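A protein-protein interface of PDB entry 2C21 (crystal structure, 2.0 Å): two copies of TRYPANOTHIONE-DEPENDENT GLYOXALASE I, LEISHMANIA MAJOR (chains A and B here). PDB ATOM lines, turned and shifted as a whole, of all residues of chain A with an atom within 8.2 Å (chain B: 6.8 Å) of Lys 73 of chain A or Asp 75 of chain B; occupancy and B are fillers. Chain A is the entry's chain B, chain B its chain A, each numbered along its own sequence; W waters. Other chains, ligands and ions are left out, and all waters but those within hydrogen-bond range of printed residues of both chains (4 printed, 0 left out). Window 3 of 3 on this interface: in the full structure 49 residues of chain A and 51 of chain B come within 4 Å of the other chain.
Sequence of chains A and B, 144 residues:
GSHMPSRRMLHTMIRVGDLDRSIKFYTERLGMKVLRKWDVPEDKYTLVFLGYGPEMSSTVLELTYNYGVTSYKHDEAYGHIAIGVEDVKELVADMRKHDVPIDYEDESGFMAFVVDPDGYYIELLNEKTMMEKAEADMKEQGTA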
ATOM      1  N   ARG A  15       0.901  26.823 -13.025  1.00  0.00           N
ATOM      2  CA  ARG A  15      -0.127  27.580 -13.732  1.00  0.00           C
ATOM      3  C   ARG A  15       0.293  29.067 -13.833  1.00  0.00           C
ATOM      4  O   ARG A  15       0.798  29.650 -12.868  1.00  0.00           O
ATOM      5  CB  ARG A  15      -1.465  27.440 -13.037  1.00  0.00           C
ATOM      6  CG  ARG A  15      -2.055  26.042 -13.098  1.00  0.00           C
ATOM      7  CD  ARG A  15      -3.259  25.948 -12.215  1.00  0.00           C
ATOM      8  NE  ARG A  15      -3.767  24.581 -12.142  1.00  0.00           N
ATOM      9  CZ  ARG A  15      -3.479  23.695 -11.199  1.00  0.00           C
ATOM     10  NH1 ARG A  15      -2.635  23.956 -10.214  1.00  0.00           N
ATOM     11  NH2 ARG A  15      -4.024  22.494 -11.274  1.00  0.00           N
ATOM     12  N   VAL A  69      -8.153  33.206 -16.440  1.00  0.00           N
ATOM     13  CA  VAL A  69      -7.551  33.265 -15.113  1.00  0.00           C
ATOM     14  C   VAL A  69      -6.255  34.040 -15.220  1.00  0.00           C
ATOM     15  O   VAL A  69      -5.262  33.562 -15.796  1.00  0.00           O
ATOM     16  CB  VAL A  69      -7.309  31.862 -14.524  1.00  0.00           C
ATOM     17  CG1 VAL A  69      -6.731  31.933 -13.134  1.00  0.00           C
ATOM     18  CG2 VAL A  69      -8.612  31.061 -14.513  1.00  0.00           C
ATOM     19  N   SER A  71      -4.157  35.495 -12.852  1.00  0.00           N
ATOM     20  CA  SER A  71      -3.164  35.540 -11.783  1.00  0.00           C
ATOM     21  C   SER A  71      -3.456  34.439 -10.785  1.00  0.00           C
ATOM     22  O   SER A  71      -4.590  33.975 -10.708  1.00  0.00           O
ATOM     23  CB  SER A  71      -3.228  36.886 -11.054  1.00  0.00           C
ATOM     24  OG  SER A  71      -2.141  37.034 -10.160  1.00  0.00           O
ATOM     25  N   TYR A  72      -2.435  34.071  -9.997  1.00  0.00           N
ATOM     26  CA  TYR A  72      -2.533  33.020  -8.984  1.00  0.00           C
ATOM     27  C   TYR A  72      -1.974  33.467  -7.618  1.00  0.00           C
ATOM     28  O   TYR A  72      -1.098  34.318  -7.535  1.00  0.00           O
ATOM     29  CB  TYR A  72      -1.783  31.769  -9.462  1.00  0.00           C
ATOM     30  CG  TYR A  72      -2.443  31.137 -10.641  1.00  0.00           C
ATOM     31  CD1 TYR A  72      -2.136  31.557 -11.941  1.00  0.00           C
ATOM     32  CD2 TYR A  72      -3.447  30.191 -10.472  1.00  0.00           C
ATOM     33  CE1 TYR A  72      -2.796  31.003 -13.042  1.00  0.00           C
ATOM     34  CE2 TYR A  72      -4.099  29.647 -11.557  1.00  0.00           C
ATOM     35  CZ  TYR A  72      -3.780  30.069 -12.849  1.00  0.00           C
ATOM     36  OH  TYR A  72      -4.450  29.525 -13.943  1.00  0.00           O
ATOM     37  N   LYS A  73      -2.516  32.887  -6.561  1.00  0.00           N
ATOM     38  CA  LYS A  73      -2.069  33.081  -5.183  1.00  0.00           C
ATOM     39  C   LYS A  73      -1.192  31.867  -4.852  1.00  0.00           C
ATOM     40  O   LYS A  73      -1.537  30.723  -5.201  1.00  0.00           O
ATOM     41  CB  LYS A  73      -3.287  33.091  -4.246  1.00  0.00           C
ATOM     42  CG  LYS A  73      -3.000  33.228  -2.771  1.00  0.00           C
ATOM     43  CD  LYS A  73      -4.295  33.212  -1.971  1.00  0.00           C
ATOM     44  CE  LYS A  73      -4.097  32.845  -0.507  1.00  0.00           C
ATOM     45  NZ  LYS A  73      -2.870  33.431   0.120  1.00  0.00           N
ATOM     46  N   HIS A  74      -0.111  32.091  -4.120  1.00  0.00           N
ATOM     47  CA  HIS A  74       0.802  30.992  -3.741  1.00  0.00           C
ATOM     48  C   HIS A  74       0.596  30.563  -2.305  1.00  0.00           C
ATOM     49  O   HIS A  74       0.387  31.408  -1.431  1.00  0.00           O
ATOM     50  CB  HIS A  74       2.218  31.429  -3.946  1.00  0.00           C
ATOM     51  CG  HIS A  74       2.488  31.803  -5.347  1.00  0.00           C
ATOM     52  ND1 HIS A  74       2.661  30.860  -6.335  1.00  0.00           N
ATOM     53  CD2 HIS A  74       2.529  33.010  -5.954  1.00  0.00           C
ATOM     54  CE1 HIS A  74       2.809  31.483  -7.491  1.00  0.00           C
ATOM     55  NE2 HIS A  74       2.760  32.783  -7.282  1.00  0.00           N
ATOM     56  N   ASP A  75       0.624  29.250  -2.087  1.00  0.00           N
ATOM     57  CA  ASP A  75       0.529  28.651  -0.762  1.00  0.00           C
ATOM     58  C   ASP A  75       1.893  28.619  -0.094  1.00  0.00           C
ATOM     59  O   ASP A  75       2.900  29.045  -0.672  1.00  0.00           O
ATOM     60  CB  ASP A  75      -0.073  27.218  -0.844  1.00  0.00           C
ATOM     61  CG  ASP A  75       0.729  26.234  -1.757  1.00  0.00           C
ATOM     62  OD1 ASP A  75       1.984  26.199  -1.775  1.00  0.00           O
ATOM     63  OD2 ASP A  75       0.063  25.443  -2.456  1.00  0.00           O
ATOM     64  N   GLU A  76       1.935  28.072   1.114  1.00  0.00           N
ATOM     65  CA  GLU A  76       3.208  27.876   1.789  1.00  0.00           C
ATOM     66  C   GLU A  76       3.712  26.441   1.641  1.00  0.00           C
ATOM     67  O   GLU A  76       4.570  26.015   2.399  1.00  0.00           O
ATOM     68  CB  GLU A  76       3.060  28.238   3.266  1.00  0.00           C
ATOM     69  CG  GLU A  76       2.404  29.611   3.468  1.00  0.00           C
ATOM     70  CD  GLU A  76       2.362  30.028   4.909  1.00  0.00           C
ATOM     71  OE1 GLU A  76       1.251  30.106   5.468  1.00  0.00           O
ATOM     72  OE2 GLU A  76       3.445  30.271   5.475  1.00  0.00           O
ATOM     73  N   ALA A  77       3.173  25.709   0.661  1.00  0.00           N
ATOM     74  CA  ALA A  77       3.464  24.294   0.478  1.00  0.00           C
ATOM     75  C   ALA A  77       4.501  24.081  -0.630  1.00  0.00           C
ATOM     76  O   ALA A  77       5.626  23.678  -0.351  1.00  0.00           O
ATOM     77  CB  ALA A  77       2.181  23.543   0.185  1.00  0.00           C
ATOM     78  N   TYR A  78       4.132  24.349  -1.876  1.00  0.00           N
ATOM     79  CA  TYR A  78       5.075  24.243  -2.990  1.00  0.00           C
ATOM     80  C   TYR A  78       6.285  25.155  -2.771  1.00  0.00           C
ATOM     81  O   TYR A  78       6.141  26.292  -2.312  1.00  0.00           O
ATOM     82  CB  TYR A  78       4.415  24.574  -4.313  1.00  0.00           C
ATOM     83  CG  TYR A  78       5.420  24.695  -5.439  1.00  0.00           C
ATOM     84  CD1 TYR A  78       6.147  23.587  -5.860  1.00  0.00           C
ATOM     85  CD2 TYR A  78       5.690  25.934  -6.043  1.00  0.00           C
ATOM     86  CE1 TYR A  78       7.081  23.686  -6.883  1.00  0.00           C
ATOM     87  CE2 TYR A  78       6.654  26.045  -7.067  1.00  0.00           C
ATOM     88  CZ  TYR A  78       7.349  24.908  -7.462  1.00  0.00           C
ATOM     89  OH  TYR A  78       8.290  24.973  -8.469  1.00  0.00           O
ATOM     90  N   GLY A  79       7.477  24.619  -3.047  1.00  0.00           N
ATOM     91  CA  GLY A  79       8.702  25.345  -2.849  1.00  0.00           C
ATOM     92  C   GLY A  79       9.192  26.109  -4.055  1.00  0.00           C
ATOM     93  O   GLY A  79       9.050  27.329  -4.132  1.00  0.00           O
ATOM     94  N   ASP A 118       4.798  35.277 -12.381  1.00  0.00           N
ATOM     95  CA  ASP A 118       3.609  34.871 -11.638  1.00  0.00           C
ATOM     96  C   ASP A 118       3.847  34.715 -10.159  1.00  0.00           C
ATOM     97  O   ASP A 118       2.935  34.319  -9.430  1.00  0.00           O
ATOM     98  CB  ASP A 118       3.058  33.582 -12.204  1.00  0.00           C
ATOM     99  CG  ASP A 118       2.409  33.802 -13.541  1.00  0.00           C
ATOM    100  OD1 ASP A 118       1.261  34.274 -13.547  1.00  0.00           O
ATOM    101  OD2 ASP A 118       3.054  33.536 -14.577  1.00  0.00           O
ATOM    102  N   GLY A 119       5.051  35.037  -9.706  1.00  0.00           N
ATOM    103  CA  GLY A 119       5.345  35.031  -8.269  1.00  0.00           C
ATOM    104  C   GLY A 119       5.933  33.738  -7.732  1.00  0.00           C
ATOM    105  O   GLY A 119       6.074  33.606  -6.523  1.00  0.00           O
ATOM    106  N   TYR A 120       6.257  32.788  -8.605  1.00  0.00           N
ATOM    107  CA  TYR A 120       6.931  31.559  -8.180  1.00  0.00           C
ATOM    108  C   TYR A 120       8.423  31.817  -7.958  1.00  0.00           C
ATOM    109  O   TYR A 120       9.009  32.687  -8.610  1.00  0.00           O
ATOM    110  CB  TYR A 120       6.807  30.445  -9.206  1.00  0.00           C
ATOM    111  CG  TYR A 120       5.432  29.965  -9.519  1.00  0.00           C
ATOM    112  CD1 TYR A 120       4.809  29.002  -8.733  1.00  0.00           C
ATOM    113  CD2 TYR A 120       4.743  30.457 -10.639  1.00  0.00           C
ATOM    114  CE1 TYR A 120       3.546  28.533  -9.049  1.00  0.00           C
ATOM    115  CE2 TYR A 120       3.488  30.006 -10.963  1.00  0.00           C
ATOM    116  CZ  TYR A 120       2.889  29.042 -10.177  1.00  0.00           C
ATOM    117  OH  TYR A 120       1.623  28.608 -10.501  1.00  0.00           O
ATOM    118  N   LYS B  73      -1.597  23.329   3.580  1.00  0.00           N
ATOM    119  CA  LYS B  73      -2.720  23.523   2.651  1.00  0.00           C
ATOM    120  C   LYS B  73      -2.205  24.006   1.297  1.00  0.00           C
ATOM    121  O   LYS B  73      -1.148  24.659   1.208  1.00  0.00           O
ATOM    122  CB  LYS B  73      -3.786  24.481   3.200  1.00  0.00           C
ATOM    123  CG  LYS B  73      -3.332  25.929   3.381  1.00  0.00           C
ATOM    124  CD  LYS B  73      -4.407  26.924   2.914  1.00  0.00           C
ATOM    125  CE  LYS B  73      -5.710  26.799   3.704  1.00  0.00           C
ATOM    126  NZ  LYS B  73      -6.888  27.287   2.907  1.00  0.00           N
ATOM    127  N   HIS B  74      -2.958  23.665   0.249  1.00  0.00           N
ATOM    128  CA  HIS B  74      -2.501  23.845  -1.116  1.00  0.00           C
ATOM    129  C   HIS B  74      -3.265  24.954  -1.829  1.00  0.00           C
ATOM    130  O   HIS B  74      -4.482  25.118  -1.631  1.00  0.00           O
ATOM    131  CB  HIS B  74      -2.633  22.552  -1.890  1.00  0.00           C
ATOM    132  CG  HIS B  74      -1.832  21.435  -1.307  1.00  0.00           C
ATOM    133  ND1 HIS B  74      -0.515  21.220  -1.635  1.00  0.00           N
ATOM    134  CD2 HIS B  74      -2.145  20.510  -0.371  1.00  0.00           C
ATOM    135  CE1 HIS B  74      -0.056  20.190  -0.947  1.00  0.00           C
ATOM    136  NE2 HIS B  74      -1.023  19.742  -0.171  1.00  0.00           N
ATOM    137  N   ASP B  75      -2.512  25.700  -2.640  1.00  0.00           N
ATOM    138  CA  ASP B  75      -3.044  26.668  -3.578  1.00  0.00           C
ATOM    139  C   ASP B  75      -3.445  25.927  -4.842  1.00  0.00           C
ATOM    140  O   ASP B  75      -3.184  24.732  -4.991  1.00  0.00           O
ATOM    141  CB  ASP B  75      -1.988  27.762  -3.921  1.00  0.00           C
ATOM    142  CG  ASP B  75      -0.680  27.192  -4.571  1.00  0.00           C
ATOM    143  OD1 ASP B  75      -0.741  26.309  -5.436  1.00  0.00           O
ATOM    144  OD2 ASP B  75       0.440  27.638  -4.219  1.00  0.00           O
ATOM    145  N   GLU B  76      -4.068  26.652  -5.754  1.00  0.00           N
ATOM    146  CA  GLU B  76      -4.370  26.115  -7.075  1.00  0.00           C
ATOM    147  C   GLU B  76      -3.446  26.750  -8.117  1.00  0.00           C
ATOM    148  O   GLU B  76      -3.869  27.020  -9.240  1.00  0.00           O
ATOM    149  CB  GLU B  76      -5.837  26.339  -7.397  1.00  0.00           C
ATOM    150  CG  GLU B  76      -6.748  25.577  -6.409  1.00  0.00           C
ATOM    151  CD  GLU B  76      -8.140  25.301  -6.958  1.00  0.00           C
ATOM    152  OE1 GLU B  76      -8.895  26.269  -7.191  1.00  0.00           O
ATOM    153  OE2 GLU B  76      -8.476  24.109  -7.135  1.00  0.00           O
ATOM    154  N   ALA B  77      -2.183  26.973  -7.714  1.00  0.00           N
ATOM    155  CA  ALA B  77      -1.159  27.587  -8.569  1.00  0.00           C
ATOM    156  C   ALA B  77      -0.200  26.491  -9.019  1.00  0.00           C
ATOM    157  O   ALA B  77      -0.160  26.153 -10.207  1.00  0.00           O
ATOM    158  CB  ALA B  77      -0.422  28.718  -7.830  1.00  0.00           C
ATOM    159  N   TYR B  78       0.551  25.936  -8.066  1.00  0.00           N
ATOM    160  CA  TYR B  78       1.424  24.824  -8.342  1.00  0.00           C
ATOM    161  C   TYR B  78       0.586  23.641  -8.889  1.00  0.00           C
ATOM    162  O   TYR B  78      -0.526  23.377  -8.419  1.00  0.00           O
ATOM    163  CB  TYR B  78       2.231  24.401  -7.113  1.00  0.00           C
ATOM    164  CG  TYR B  78       2.934  23.089  -7.324  1.00  0.00           C
ATOM    165  CD1 TYR B  78       4.027  23.001  -8.179  1.00  0.00           C
ATOM    166  CD2 TYR B  78       2.468  21.919  -6.720  1.00  0.00           C
ATOM    167  CE1 TYR B  78       4.666  21.783  -8.409  1.00  0.00           C
ATOM    168  CE2 TYR B  78       3.106  20.687  -6.941  1.00  0.00           C
ATOM    169  CZ  TYR B  78       4.191  20.633  -7.790  1.00  0.00           C
ATOM    170  OH  TYR B  78       4.810  19.444  -7.988  1.00  0.00           O
ATOM    171  N   GLY B  79       1.130  22.959  -9.881  1.00  0.00           N
ATOM    172  CA  GLY B  79       0.405  21.921 -10.599  1.00  0.00           C
ATOM    173  C   GLY B  79       0.714  20.548 -10.081  1.00  0.00           C
ATOM    174  O   GLY B  79      -0.051  19.973  -9.298  1.00  0.00           O
HETATM  175  O   HOH W   1       2.634  28.212  -5.384  1.00  0.00           O
HETATM  176  O   HOH W   2       0.120  26.350   2.465  1.00  0.00           O
HETATM  177  O   HOH W   3       0.557  23.093  -3.361  1.00  0.00           O
HETATM  178  O   HOH W   4      -2.706  20.882  -8.806  1.00  0.00           O
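N of Asp 75 of chain B is in hydrogen-bond range of OD2 of Asp 75 of chain A (2.6 Å).
The backbone carbonyl oxygen of Glu 76 of chain B lies close to the guanidinium group of Arg 15 of chain A (3.4 Å).
O of Ala 77 of chain B lies within hydrogen-bond range of N of Arg 15 of chain A, 3.1 Å away.
The backbone carbonyl oxygen (O) of Ala 77 of chain B lies within hydrogen-bond range of the side-chain hydroxyl (OH) of Tyr 120 of chain A (3.0 Å).
O of Tyr 78 of chain B is in hydrogen-bond range of NH1 of Arg 15 of chain A, 2.8 Å away.
Of the printed residues of chain B, Lys 73 of chain A touches Asp 75 (3.3 Å) and Ala 77 (3.5 Å).
Asp 75 of chain B touches just these residues of chain A: Lys 73 (3.3 Å), His 74 (3.4 Å) and Asp 75 (2.6 Å).
Of the printed residues of chain A, His 74 of chain B touches Asp 75 (3.3 Å) and Ala 77 (3.997 Å).
Printed residues of chain B within 4 Å of Asp 75 of chain A: Lys 73, His 74 and Asp 75.
Printed residues of chain A within 4 Å of Ala 77 of chain B: Arg 15, Tyr 72, Lys 73 and Tyr 120.
Of the printed residues of chain B, Tyr 120 of chain A touches Ala 77 (3.0 Å) and Tyr 78 (3.8 Å).
Of the printed residues of chain B, Tyr 78 of chain A touches Tyr 78.
Asp 118 of chain A touches none of the printed residues of chain B.
The nearest printed residue of chain A that does not touch Ala 77 of chain B is His 74 of chain A (4.04 Å).
Among the printed residues, merely in contact across the chains: Tyr 78 of chain A with Tyr 78 of chain B, Lys 73 of chain A with Asp 75 of chain B, Asp 75 of chain A with His 74 of chain B, His 74 of chain A with Asp 75 of chain B, Tyr 72 of chain A with Glu 76 of chain B, Asp 75 of chain A with Lys 73 of chain B, Lys 73 of chain A with Ala 77 of chain B, Ala 77 of chain A with Lys 73 of chain B, Arg 15 of chain A with Gly 79 of chain B, Tyr 72 of chain A with Ala 77 of chain B, Tyr 120 of chain A with Tyr 78 of chain B and Ala 77 of chain A with His 74 of chain B.
Lys 73 of chain A touches Asp 75 of chain B, and with the chains exchanged Asp 75 of chain A touches Lys 73 of chain B.
Lys 73 of chain A touches Ala 77 of chain B, and with the chains exchanged Ala 77 of chain A touches Lys 73 of chain B.
Ala 77 of chain A touches His 74 of chain B, but with the chains exchanged His 74 of chain A does not touch Ala 77 of chain B (4.04 Å).
Tyr 78 of chain B touches its own counterpart, Tyr 78 of chain A.
7 positions are printed for both chains.
Of the 17 pairs that touch across the chains among the printed residues, 8 have their exchanged pair printed and touching as well.
The side-chain carboxylate of Asp 75 of chain B sits at hydrogen-bond distance from the backbone NH of Ala 77 of chain B (2.8 Å).
The backbone NH (N) of Tyr 78 of chain B sits at hydrogen-bond distance from the side-chain carboxylate (OD1) of Asp 75 of chain B (3.0 Å).
OH of Tyr 120 of chain A is in hydrogen-bond range of O of Arg 15 of chain A, at 2.7 Å.
The backbone carbonyl oxygen (O) of Asp 118 of chain A sits at hydrogen-bond distance from a ring nitrogen (NE2) of His 74 of chain A (2.6 Å).
The backbone carbonyl oxygen (O) of Gly 119 of chain A lies close to a ring nitrogen (NE2) of His 74 of chain A.
N of Tyr 78 of chain A sits at hydrogen-bond distance from OD1 of Asp 75 of chain A (2.8 Å).
Water W2 bridges O of Lys 73 of chain B (2.5 Å) and N of Glu 76 of chain A (2.8 Å).
Water W1 bridges the side-chain carboxylate (OD2) of Asp 75 of chain B (2.5 Å) and a ring nitrogen (ND1) of His 74 of chain A (2.8 Å).
Water W3 lies within hydrogen-bond range of OD2 of Asp 75 of chain A (2.6 Å) and ND1 of His 74 of chain B (2.8 Å).
Water W4 lies within hydrogen-bond range of O of Gly 79 of chain B (2.8 Å), NH2 of Arg 15 of chain A (3.2 Å) and O of Tyr 78 of chain B (3.3 Å).
Printed residues of chain A that touch a printed residue of chain B: Arg 15, Tyr 72, Lys 73, His 74, Asp 75, Ala 77, Tyr 78 and Tyr 120.
Hydrophobic or aromatic side chains of chain A that line the printed part of chain B: Tyr 72, Ala 77, Tyr 78 and Tyr 120.
Printed residues of chain B that touch a printed residue of chain A: Lys 73, His 74, Asp 75, Glu 76, Ala 77, Tyr 78 and Gly 79.
Along chain B the printed residues that touch a printed residue of chain A span positions 73 to 79.
Among the printed residues, 17 pairs touch across the chains.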
